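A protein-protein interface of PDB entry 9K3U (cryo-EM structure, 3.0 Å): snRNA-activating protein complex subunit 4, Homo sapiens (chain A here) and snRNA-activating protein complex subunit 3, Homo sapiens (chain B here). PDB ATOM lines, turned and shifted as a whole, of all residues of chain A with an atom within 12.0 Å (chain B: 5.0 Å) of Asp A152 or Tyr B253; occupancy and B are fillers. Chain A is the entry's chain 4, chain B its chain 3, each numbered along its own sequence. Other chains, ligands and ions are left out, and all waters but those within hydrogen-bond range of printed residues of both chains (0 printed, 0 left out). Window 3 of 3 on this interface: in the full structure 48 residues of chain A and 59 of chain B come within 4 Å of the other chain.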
ATOM      1  N   PRO A 148      14.408   3.725  10.291  1.00  0.00           N
ATOM      2  CA  PRO A 148      15.160   2.712  11.035  1.00  0.00           C
ATOM      3  C   PRO A 148      16.207   3.314  11.967  1.00  0.00           C
ATOM      4  O   PRO A 148      16.537   4.493  11.844  1.00  0.00           O
ATOM      5  CB  PRO A 148      15.823   1.892   9.925  1.00  0.00           C
ATOM      6  CG  PRO A 148      14.962   2.111   8.690  1.00  0.00           C
ATOM      7  CD  PRO A 148      13.976   3.219   8.982  1.00  0.00           C
ATOM      8  N   TYR A 149      16.720   2.502  12.887  1.00  0.00           N
ATOM      9  CA  TYR A 149      17.732   2.937  13.837  1.00  0.00           C
ATOM     10  C   TYR A 149      18.819   1.877  13.931  1.00  0.00           C
ATOM     11  O   TYR A 149      18.549   0.678  13.830  1.00  0.00           O
ATOM     12  CB  TYR A 149      17.128   3.198  15.225  1.00  0.00           C
ATOM     13  CG  TYR A 149      16.274   2.063  15.740  1.00  0.00           C
ATOM     14  CD1 TYR A 149      16.831   1.021  16.468  1.00  0.00           C
ATOM     15  CD2 TYR A 149      14.906   2.036  15.500  1.00  0.00           C
ATOM     16  CE1 TYR A 149      16.052  -0.017  16.941  1.00  0.00           C
ATOM     17  CE2 TYR A 149      14.118   1.002  15.968  1.00  0.00           C
ATOM     18  CZ  TYR A 149      14.696  -0.020  16.689  1.00  0.00           C
ATOM     19  OH  TYR A 149      13.914  -1.053  17.156  1.00  0.00           O
ATOM     20  N   PHE A 150      20.056   2.335  14.125  1.00  0.00           N
ATOM     21  CA  PHE A 150      21.214   1.456  14.221  1.00  0.00           C
ATOM     22  C   PHE A 150      21.952   1.741  15.531  1.00  0.00           C
ATOM     23  O   PHE A 150      23.174   1.832  15.592  1.00  0.00           O
ATOM     24  CB  PHE A 150      22.125   1.631  13.008  1.00  0.00           C
ATOM     25  CG  PHE A 150      21.428   1.421  11.695  1.00  0.00           C
ATOM     26  CD1 PHE A 150      21.236   0.145  11.192  1.00  0.00           C
ATOM     27  CD2 PHE A 150      20.964   2.500  10.962  1.00  0.00           C
ATOM     28  CE1 PHE A 150      20.593  -0.051   9.985  1.00  0.00           C
ATOM     29  CE2 PHE A 150      20.321   2.310   9.754  1.00  0.00           C
ATOM     30  CZ  PHE A 150      20.135   1.033   9.265  1.00  0.00           C
ATOM     31  N   LYS A 151      21.175   1.889  16.614  1.00  0.00           N
ATOM     32  CA  LYS A 151      21.757   2.115  17.933  1.00  0.00           C
ATOM     33  C   LYS A 151      21.107   1.238  19.001  1.00  0.00           C
ATOM     34  O   LYS A 151      20.729   1.754  20.057  1.00  0.00           O
ATOM     35  CB  LYS A 151      21.623   3.597  18.327  1.00  0.00           C
ATOM     36  CG  LYS A 151      22.259   4.573  17.338  1.00  0.00           C
ATOM     37  CD  LYS A 151      23.781   4.479  17.321  1.00  0.00           C
ATOM     38  CE  LYS A 151      24.399   5.073  18.580  1.00  0.00           C
ATOM     39  NZ  LYS A 151      25.888   5.065  18.534  1.00  0.00           N
ATOM     40  N   ASP A 152      20.958  -0.066  18.750  1.00  0.00           N
ATOM     41  CA  ASP A 152      20.234  -0.950  19.657  1.00  0.00           C
ATOM     42  C   ASP A 152      20.784  -0.900  21.080  1.00  0.00           C
ATOM     43  O   ASP A 152      20.076  -0.523  22.019  1.00  0.00           O
ATOM     44  CB  ASP A 152      20.288  -2.384  19.114  1.00  0.00           C
ATOM     45  CG  ASP A 152      19.551  -3.369  19.999  1.00  0.00           C
ATOM     46  OD1 ASP A 152      18.303  -3.308  20.047  1.00  0.00           O
ATOM     47  OD2 ASP A 152      20.217  -4.203  20.644  1.00  0.00           O
ATOM     48  N   LYS A 153      22.049  -1.284  21.254  1.00  0.00           N
ATOM     49  CA  LYS A 153      22.618  -1.394  22.592  1.00  0.00           C
ATOM     50  C   LYS A 153      22.827  -0.022  23.222  1.00  0.00           C
ATOM     51  O   LYS A 153      22.226   0.298  24.256  1.00  0.00           O
ATOM     52  CB  LYS A 153      23.939  -2.166  22.533  1.00  0.00           C
ATOM     53  CG  LYS A 153      24.687  -2.239  23.857  1.00  0.00           C
ATOM     54  CD  LYS A 153      25.950  -3.075  23.738  1.00  0.00           C
ATOM     55  CE  LYS A 153      25.635  -4.561  23.661  1.00  0.00           C
ATOM     56  NZ  LYS A 153      26.864  -5.381  23.490  1.00  0.00           N
ATOM     57  N   VAL A 154      23.674   0.802  22.612  1.00  0.00           N
ATOM     58  CA  VAL A 154      23.959   2.143  23.115  1.00  0.00           C
ATOM     59  C   VAL A 154      22.997   3.098  22.415  1.00  0.00           C
ATOM     60  O   VAL A 154      23.174   3.434  21.244  1.00  0.00           O
ATOM     61  CB  VAL A 154      25.422   2.537  22.900  1.00  0.00           C
ATOM     62  CG1 VAL A 154      26.308   1.842  23.925  1.00  0.00           C
ATOM     63  CG2 VAL A 154      25.887   2.200  21.486  1.00  0.00           C
ATOM     64  N   THR A 155      21.963   3.530  23.142  1.00  0.00           N
ATOM     65  CA  THR A 155      20.959   4.411  22.553  1.00  0.00           C
ATOM     66  C   THR A 155      21.596   5.651  21.939  1.00  0.00           C
ATOM     67  O   THR A 155      21.150   6.137  20.893  1.00  0.00           O
ATOM     68  CB  THR A 155      19.927   4.812  23.611  1.00  0.00           C
ATOM     69  OG1 THR A 155      20.589   5.450  24.710  1.00  0.00           O
ATOM     70  CG2 THR A 155      19.177   3.585  24.115  1.00  0.00           C
ATOM     71  N   GLY A 156      22.641   6.175  22.574  1.00  0.00           N
ATOM     72  CA  GLY A 156      23.332   7.344  22.068  1.00  0.00           C
ATOM     73  C   GLY A 156      23.511   8.426  23.112  1.00  0.00           C
ATOM     74  O   GLY A 156      23.958   9.534  22.796  1.00  0.00           O
ATOM     75  N   VAL A 157      23.169   8.122  24.360  1.00  0.00           N
ATOM     76  CA  VAL A 157      23.293   9.095  25.441  1.00  0.00           C
ATOM     77  C   VAL A 157      24.652   8.992  26.124  1.00  0.00           C
ATOM     78  O   VAL A 157      25.242  10.008  26.497  1.00  0.00           O
ATOM     79  CB  VAL A 157      22.138   8.917  26.448  1.00  0.00           C
ATOM     80  CG1 VAL A 157      22.220   7.561  27.143  1.00  0.00           C
ATOM     81  CG2 VAL A 157      22.140  10.049  27.465  1.00  0.00           C
ATOM     82  N   GLY A 158      25.168   7.777  26.300  1.00  0.00           N
ATOM     83  CA  GLY A 158      26.434   7.577  26.965  1.00  0.00           C
ATOM     84  C   GLY A 158      27.328   6.542  26.308  1.00  0.00           C
ATOM     85  O   GLY A 158      28.017   5.782  26.994  1.00  0.00           O
ATOM     86  N   PRO A 159      27.342   6.482  24.978  1.00  0.00           N
ATOM     87  CA  PRO A 159      28.137   5.455  24.293  1.00  0.00           C
ATOM     88  C   PRO A 159      29.608   5.577  24.650  1.00  0.00           C
ATOM     89  O   PRO A 159      30.248   6.591  24.330  1.00  0.00           O
ATOM     90  CB  PRO A 159      27.896   5.752  22.806  1.00  0.00           C
ATOM     91  CG  PRO A 159      27.569   7.196  22.764  1.00  0.00           C
ATOM     92  CD  PRO A 159      26.804   7.472  24.025  1.00  0.00           C
ATOM     93  N   PRO A 160      30.185   4.573  25.314  1.00  0.00           N
ATOM     94  CA  PRO A 160      31.594   4.673  25.719  1.00  0.00           C
ATOM     95  C   PRO A 160      32.529   4.300  24.576  1.00  0.00           C
ATOM     96  O   PRO A 160      32.289   3.333  23.849  1.00  0.00           O
ATOM     97  CB  PRO A 160      31.701   3.675  26.875  1.00  0.00           C
ATOM     98  CG  PRO A 160      30.695   2.628  26.536  1.00  0.00           C
ATOM     99  CD  PRO A 160      29.565   3.329  25.811  1.00  0.00           C
ATOM    100  N   PHE B 251      31.494  -9.608  19.675  1.00  0.00           N
ATOM    101  CA  PHE B 251      30.565 -10.111  20.674  1.00  0.00           C
ATOM    102  C   PHE B 251      29.132  -9.840  20.239  1.00  0.00           C
ATOM    103  O   PHE B 251      28.822  -8.794  19.661  1.00  0.00           O
ATOM    104  CB  PHE B 251      30.827  -9.476  22.047  1.00  0.00           C
ATOM    105  CG  PHE B 251      30.852  -7.976  22.027  1.00  0.00           C
ATOM    106  CD1 PHE B 251      32.003  -7.292  21.667  1.00  0.00           C
ATOM    107  CD2 PHE B 251      29.728  -7.243  22.374  1.00  0.00           C
ATOM    108  CE1 PHE B 251      32.030  -5.914  21.650  1.00  0.00           C
ATOM    109  CE2 PHE B 251      29.751  -5.862  22.358  1.00  0.00           C
ATOM    110  CZ  PHE B 251      30.904  -5.198  21.996  1.00  0.00           C
ATOM    111  N   PHE B 252      28.261 -10.800  20.536  1.00  0.00           N
ATOM    112  CA  PHE B 252      26.832 -10.680  20.300  1.00  0.00           C
ATOM    113  C   PHE B 252      26.133 -10.182  21.558  1.00  0.00           C
ATOM    114  O   PHE B 252      26.682 -10.244  22.661  1.00  0.00           O
ATOM    115  CB  PHE B 252      26.233 -12.023  19.875  1.00  0.00           C
ATOM    116  CG  PHE B 252      26.555 -12.417  18.459  1.00  0.00           C
ATOM    117  CD1 PHE B 252      27.711 -13.122  18.168  1.00  0.00           C
ATOM    118  CD2 PHE B 252      25.697 -12.089  17.423  1.00  0.00           C
ATOM    119  CE1 PHE B 252      28.005 -13.490  16.867  1.00  0.00           C
ATOM    120  CE2 PHE B 252      25.988 -12.454  16.123  1.00  0.00           C
ATOM    121  CZ  PHE B 252      27.143 -13.156  15.845  1.00  0.00           C
ATOM    122  N   TYR B 253      24.911  -9.687  21.380  1.00  0.00           N
ATOM    123  CA  TYR B 253      24.094  -9.187  22.481  1.00  0.00           C
ATOM    124  C   TYR B 253      22.640  -9.506  22.168  1.00  0.00           C
ATOM    125  O   TYR B 253      22.056  -8.917  21.247  1.00  0.00           O
ATOM    126  CB  TYR B 253      24.296  -7.686  22.683  1.00  0.00           C
ATOM    127  CG  TYR B 253      23.247  -7.023  23.548  1.00  0.00           C
ATOM    128  CD1 TYR B 253      23.382  -6.982  24.928  1.00  0.00           C
ATOM    129  CD2 TYR B 253      22.121  -6.438  22.984  1.00  0.00           C
ATOM    130  CE1 TYR B 253      22.427  -6.375  25.723  1.00  0.00           C
ATOM    131  CE2 TYR B 253      21.159  -5.831  23.768  1.00  0.00           C
ATOM    132  CZ  TYR B 253      21.315  -5.803  25.136  1.00  0.00           C
ATOM    133  OH  TYR B 253      20.361  -5.199  25.921  1.00  0.00           O
ATOM    134  N   PHE B 254      22.071 -10.441  22.934  1.00  0.00           N
ATOM    135  CA  PHE B 254      20.687 -10.887  22.791  1.00  0.00           C
ATOM    136  C   PHE B 254      20.029 -10.853  24.164  1.00  0.00           C
ATOM    137  O   PHE B 254      20.420 -11.611  25.059  1.00  0.00           O
ATOM    138  CB  PHE B 254      20.616 -12.299  22.205  1.00  0.00           C
ATOM    139  CG  PHE B 254      21.033 -12.395  20.764  1.00  0.00           C
ATOM    140  CD1 PHE B 254      22.368 -12.498  20.419  1.00  0.00           C
ATOM    141  CD2 PHE B 254      20.083 -12.395  19.758  1.00  0.00           C
ATOM    142  CE1 PHE B 254      22.749 -12.592  19.095  1.00  0.00           C
ATOM    143  CE2 PHE B 254      20.459 -12.487  18.433  1.00  0.00           C
ATOM    144  CZ  PHE B 254      21.794 -12.586  18.101  1.00  0.00           C
ATOM    145  N   GLU B 255      19.031  -9.987  24.329  1.00  0.00           N
ATOM    146  CA  GLU B 255      18.242  -9.916  25.559  1.00  0.00           C
ATOM    147  C   GLU B 255      19.142  -9.812  26.791  1.00  0.00           C
ATOM    148  O   GLU B 255      19.043 -10.598  27.734  1.00  0.00           O
ATOM    149  CB  GLU B 255      17.310 -11.124  25.675  1.00  0.00           C
ATOM    150  CG  GLU B 255      16.271 -11.229  24.569  1.00  0.00           C
ATOM    151  CD  GLU B 255      15.294 -10.069  24.568  1.00  0.00           C
ATOM    152  OE1 GLU B 255      15.279  -9.298  25.551  1.00  0.00           O
ATOM    153  OE2 GLU B 255      14.536  -9.929  23.585  1.00  0.00           O
ATOM    154  N   GLY B 256      20.030  -8.823  26.774  1.00  0.00           N
ATOM    155  CA  GLY B 256      20.885  -8.578  27.919  1.00  0.00           C
ATOM    156  C   GLY B 256      21.953  -9.617  28.164  1.00  0.00           C
ATOM    157  O   GLY B 256      22.605  -9.575  29.211  1.00  0.00           O
ATOM    158  N   THR B 257      22.155 -10.550  27.238  1.00  0.00           N
ATOM    159  CA  THR B 257      23.173 -11.586  27.364  1.00  0.00           C
ATOM    160  C   THR B 257      24.322 -11.266  26.421  1.00  0.00           C
ATOM    161  O   THR B 257      24.110 -11.073  25.218  1.00  0.00           O
ATOM    162  CB  THR B 257      22.595 -12.968  27.051  1.00  0.00           C
ATOM    163  OG1 THR B 257      21.417 -13.187  27.836  1.00  0.00           O
ATOM    164  CG2 THR B 257      23.615 -14.055  27.360  1.00  0.00           C
ATOM    165  N   PHE B 258      25.535 -11.217  26.964  1.00  0.00           N
ATOM    166  CA  PHE B 258      26.734 -10.842  26.217  1.00  0.00           C
ATOM    167  C   PHE B 258      27.532 -12.100  25.907  1.00  0.00           C
ATOM    168  O   PHE B 258      28.121 -12.706  26.809  1.00  0.00           O
ATOM    169  CB  PHE B 258      27.576  -9.840  27.008  1.00  0.00           C
ATOM    170  CG  PHE B 258      26.939  -8.486  27.148  1.00  0.00           C
ATOM    171  CD1 PHE B 258      25.853  -8.299  27.988  1.00  0.00           C
ATOM    172  CD2 PHE B 258      27.434  -7.398  26.449  1.00  0.00           C
ATOM    173  CE1 PHE B 258      25.268  -7.052  28.118  1.00  0.00           C
ATOM    174  CE2 PHE B 258      26.854  -6.151  26.580  1.00  0.00           C
ATOM    175  CZ  PHE B 258      25.770  -5.977  27.415  1.00  0.00           C
ATOM    176  N   TYR B 259      27.555 -12.489  24.634  1.00  0.00           N
ATOM    177  CA  TYR B 259      28.345 -13.627  24.175  1.00  0.00           C
ATOM    178  C   TYR B 259      29.639 -13.099  23.566  1.00  0.00           C
ATOM    179  O   TYR B 259      29.621 -12.473  22.501  1.00  0.00           O
ATOM    180  CB  TYR B 259      27.565 -14.457  23.162  1.00  0.00           C
ATOM    181  CG  TYR B 259      26.157 -14.801  23.599  1.00  0.00           C
ATOM    182  CD1 TYR B 259      25.907 -15.922  24.383  1.00  0.00           C
ATOM    183  CD2 TYR B 259      25.081 -14.008  23.231  1.00  0.00           C
ATOM    184  CE1 TYR B 259      24.625 -16.239  24.786  1.00  0.00           C
ATOM    185  CE2 TYR B 259      23.795 -14.318  23.628  1.00  0.00           C
ATOM    186  CZ  TYR B 259      23.573 -15.433  24.405  1.00  0.00           C
ATOM    187  OH  TYR B 259      22.292 -15.745  24.804  1.00  0.00           O
ATOM    188  N   PHE B 288      23.328  -7.668  33.597  1.00  0.00           N
ATOM    189  CA  PHE B 288      23.461  -8.421  32.360  1.00  0.00           C
ATOM    190  C   PHE B 288      24.424  -9.583  32.562  1.00  0.00           C
ATOM    191  O   PHE B 288      25.435  -9.448  33.261  1.00  0.00           O
ATOM    192  CB  PHE B 288      23.964  -7.528  31.223  1.00  0.00           C
ATOM    193  CG  PHE B 288      23.050  -6.376  30.901  1.00  0.00           C
ATOM    194  CD1 PHE B 288      21.678  -6.489  31.061  1.00  0.00           C
ATOM    195  CD2 PHE B 288      23.565  -5.179  30.435  1.00  0.00           C
ATOM    196  CE1 PHE B 288      20.841  -5.432  30.765  1.00  0.00           C
ATOM    197  CE2 PHE B 288      22.732  -4.118  30.136  1.00  0.00           C
ATOM    198  CZ  PHE B 288      21.369  -4.243  30.301  1.00  0.00           C
ATOM    199  N   PHE B 307      12.630  -8.703  16.912  1.00  0.00           N
ATOM    200  CA  PHE B 307      13.240  -7.758  17.838  1.00  0.00           C
ATOM    201  C   PHE B 307      14.712  -7.557  17.497  1.00  0.00           C
ATOM    202  O   PHE B 307      15.424  -8.530  17.226  1.00  0.00           O
ATOM    203  CB  PHE B 307      13.114  -8.255  19.277  1.00  0.00           C
ATOM    204  CG  PHE B 307      13.530  -7.243  20.307  1.00  0.00           C
ATOM    205  CD1 PHE B 307      12.619  -6.324  20.800  1.00  0.00           C
ATOM    206  CD2 PHE B 307      14.833  -7.209  20.779  1.00  0.00           C
ATOM    207  CE1 PHE B 307      12.998  -5.392  21.747  1.00  0.00           C
ATOM    208  CE2 PHE B 307      15.216  -6.279  21.728  1.00  0.00           C
ATOM    209  CZ  PHE B 307      14.298  -5.370  22.212  1.00  0.00           C
ATOM    210  N   PRO B 308      15.215  -6.319  17.500  1.00  0.00           N
ATOM    211  CA  PRO B 308      16.611  -6.090  17.102  1.00  0.00           C
ATOM    212  C   PRO B 308      17.582  -6.424  18.228  1.00  0.00           C
ATOM    213  O   PRO B 308      17.406  -5.991  19.370  1.00  0.00           O
ATOM    214  CB  PRO B 308      16.642  -4.595  16.766  1.00  0.00           C
ATOM    215  CG  PRO B 308      15.594  -4.006  17.640  1.00  0.00           C
ATOM    216  CD  PRO B 308      14.512  -5.055  17.783  1.00  0.00           C
ATOM    217  N   TYR B 309      18.606  -7.203  17.895  1.00  0.00           N
ATOM    218  CA  TYR B 309      19.714  -7.532  18.780  1.00  0.00           C
ATOM    219  C   TYR B 309      21.000  -6.989  18.162  1.00  0.00           C
ATOM    220  O   TYR B 309      20.999  -6.498  17.033  1.00  0.00           O
ATOM    221  CB  TYR B 309      19.776  -9.043  19.010  1.00  0.00           C
ATOM    222  CG  TYR B 309      18.481  -9.608  19.544  1.00  0.00           C
ATOM    223  CD1 TYR B 309      18.075  -9.352  20.847  1.00  0.00           C
ATOM    224  CD2 TYR B 309      17.662 -10.398  18.748  1.00  0.00           C
ATOM    225  CE1 TYR B 309      16.895  -9.861  21.341  1.00  0.00           C
ATOM    226  CE2 TYR B 309      16.476 -10.916  19.235  1.00  0.00           C
ATOM    227  CZ  TYR B 309      16.098 -10.642  20.532  1.00  0.00           C
ATOM    228  OH  TYR B 309      14.920 -11.153  21.029  1.00  0.00           O
ATOM    229  N   LEU B 310      22.110  -7.072  18.894  1.00  0.00           N
ATOM    230  CA  LEU B 310      23.342  -6.436  18.445  1.00  0.00           C
ATOM    231  C   LEU B 310      24.423  -7.467  18.153  1.00  0.00           C
ATOM    232  O   LEU B 310      24.490  -8.520  18.794  1.00  0.00           O
ATOM    233  CB  LEU B 310      23.867  -5.435  19.482  1.00  0.00           C
ATOM    234  CG  LEU B 310      24.938  -4.464  18.974  1.00  0.00           C
ATOM    235  CD1 LEU B 310      24.300  -3.202  18.411  1.00  0.00           C
ATOM    236  CD2 LEU B 310      25.935  -4.130  20.073  1.00  0.00           C
ATOM    237  N   TYR B 311      25.271  -7.151  17.175  1.00  0.00           N
ATOM    238  CA  TYR B 311      26.506  -7.895  16.937  1.00  0.00           C
ATOM    239  C   TYR B 311      27.610  -6.874  16.699  1.00  0.00           C
ATOM    240  O   TYR B 311      27.681  -6.281  15.620  1.00  0.00           O
ATOM    241  CB  TYR B 311      26.371  -8.845  15.745  1.00  0.00           C
ATOM    242  CG  TYR B 311      27.696  -9.328  15.196  1.00  0.00           C
ATOM    243  CD1 TYR B 311      28.501 -10.189  15.929  1.00  0.00           C
ATOM    244  CD2 TYR B 311      28.139  -8.922  13.944  1.00  0.00           C
ATOM    245  CE1 TYR B 311      29.711 -10.633  15.431  1.00  0.00           C
ATOM    246  CE2 TYR B 311      29.348  -9.361  13.438  1.00  0.00           C
ATOM    247  CZ  TYR B 311      30.131 -10.215  14.186  1.00  0.00           C
ATOM    248  OH  TYR B 311      31.335 -10.655  13.687  1.00  0.00           O
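The side-chain carboxylate (OD1) of Asp A152 lies close to the backbone carbonyl oxygen (O) of Pro B308.
The backbone carbonyl oxygen (O) of Leu B310 is in hydrogen-bond range of the backbone NH (N) of Tyr B253 (2.9 Å). The side-chain carboxylate (OE2) of Glu B255 is in hydrogen-bond range of the side-chain hydroxyl (OH) of Tyr B309 (2.9 Å).
Among the printed residues, pairs that only touch across the chains: Tyr A149 with Pro B308 (3.4 Å), Asp A152 with Tyr B253 (3.6 Å), Asp A152 with Tyr B309 (3.8 Å), Asp A152 with Leu B310 (3.9 Å), Lys A153 with Phe B251 (3.1 Å), Lys A153 with Tyr B253 (3.4 Å), Lys A153 with Phe B258 (3.2 Å) and Lys A153 with Leu B310 (3.6 Å).
Of chain B, only Tyr B253, Pro B308, Tyr B309 and Leu B310 come within 4 Å of Asp A152. Tyr B253 touches just these residues of chain A: Asp A152 and Lys A153. Glu B255 touches none of the printed residues of chain A. No residue of chain A comes within 4 Å of Gly B256. No residue of chain A comes within 4 Å of Tyr B259. Of chain A, only Tyr A149 and Asp A152 come within 4 Å of Pro B308. Of chain A, only Asp A152 comes within 4 Å of Tyr B309. Of the printed residues of chain B, Tyr A149 touches Pro B308 (3.4 Å). Of the printed residues of chain A, Phe B251 touches Lys A153 (3.1 Å). Phe A150 touches none of the printed residues of chain B. Val A154 touches none of the printed residues of chain B. The nearest printed residue of chain B that does not touch Tyr A149 is Phe B307 (6.4 Å).
Of the 13 printed residues of chain A, 3 touch a printed residue of chain B. Hydrophobic or aromatic side chains of chain A within 4 Å of the printed part of chain B: Tyr A149. Of the 15 printed residues of chain B, 6 touch a printed residue of chain A. Hydrophobic or aromatic side chains of chain B within 4 Å of the printed part of chain A: Phe B251, Tyr B253, Phe B258, Pro B308 and Leu B310. Along chain B the printed residues that touch a printed residue of chain A span positions 251 to 310. Among the printed residues, 9 pairs touch across the chains. Among the printed residues, no Asp or Glu carboxylate lies within 4 Å of a Lys or Arg side-chain nitrogen of the other chain.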
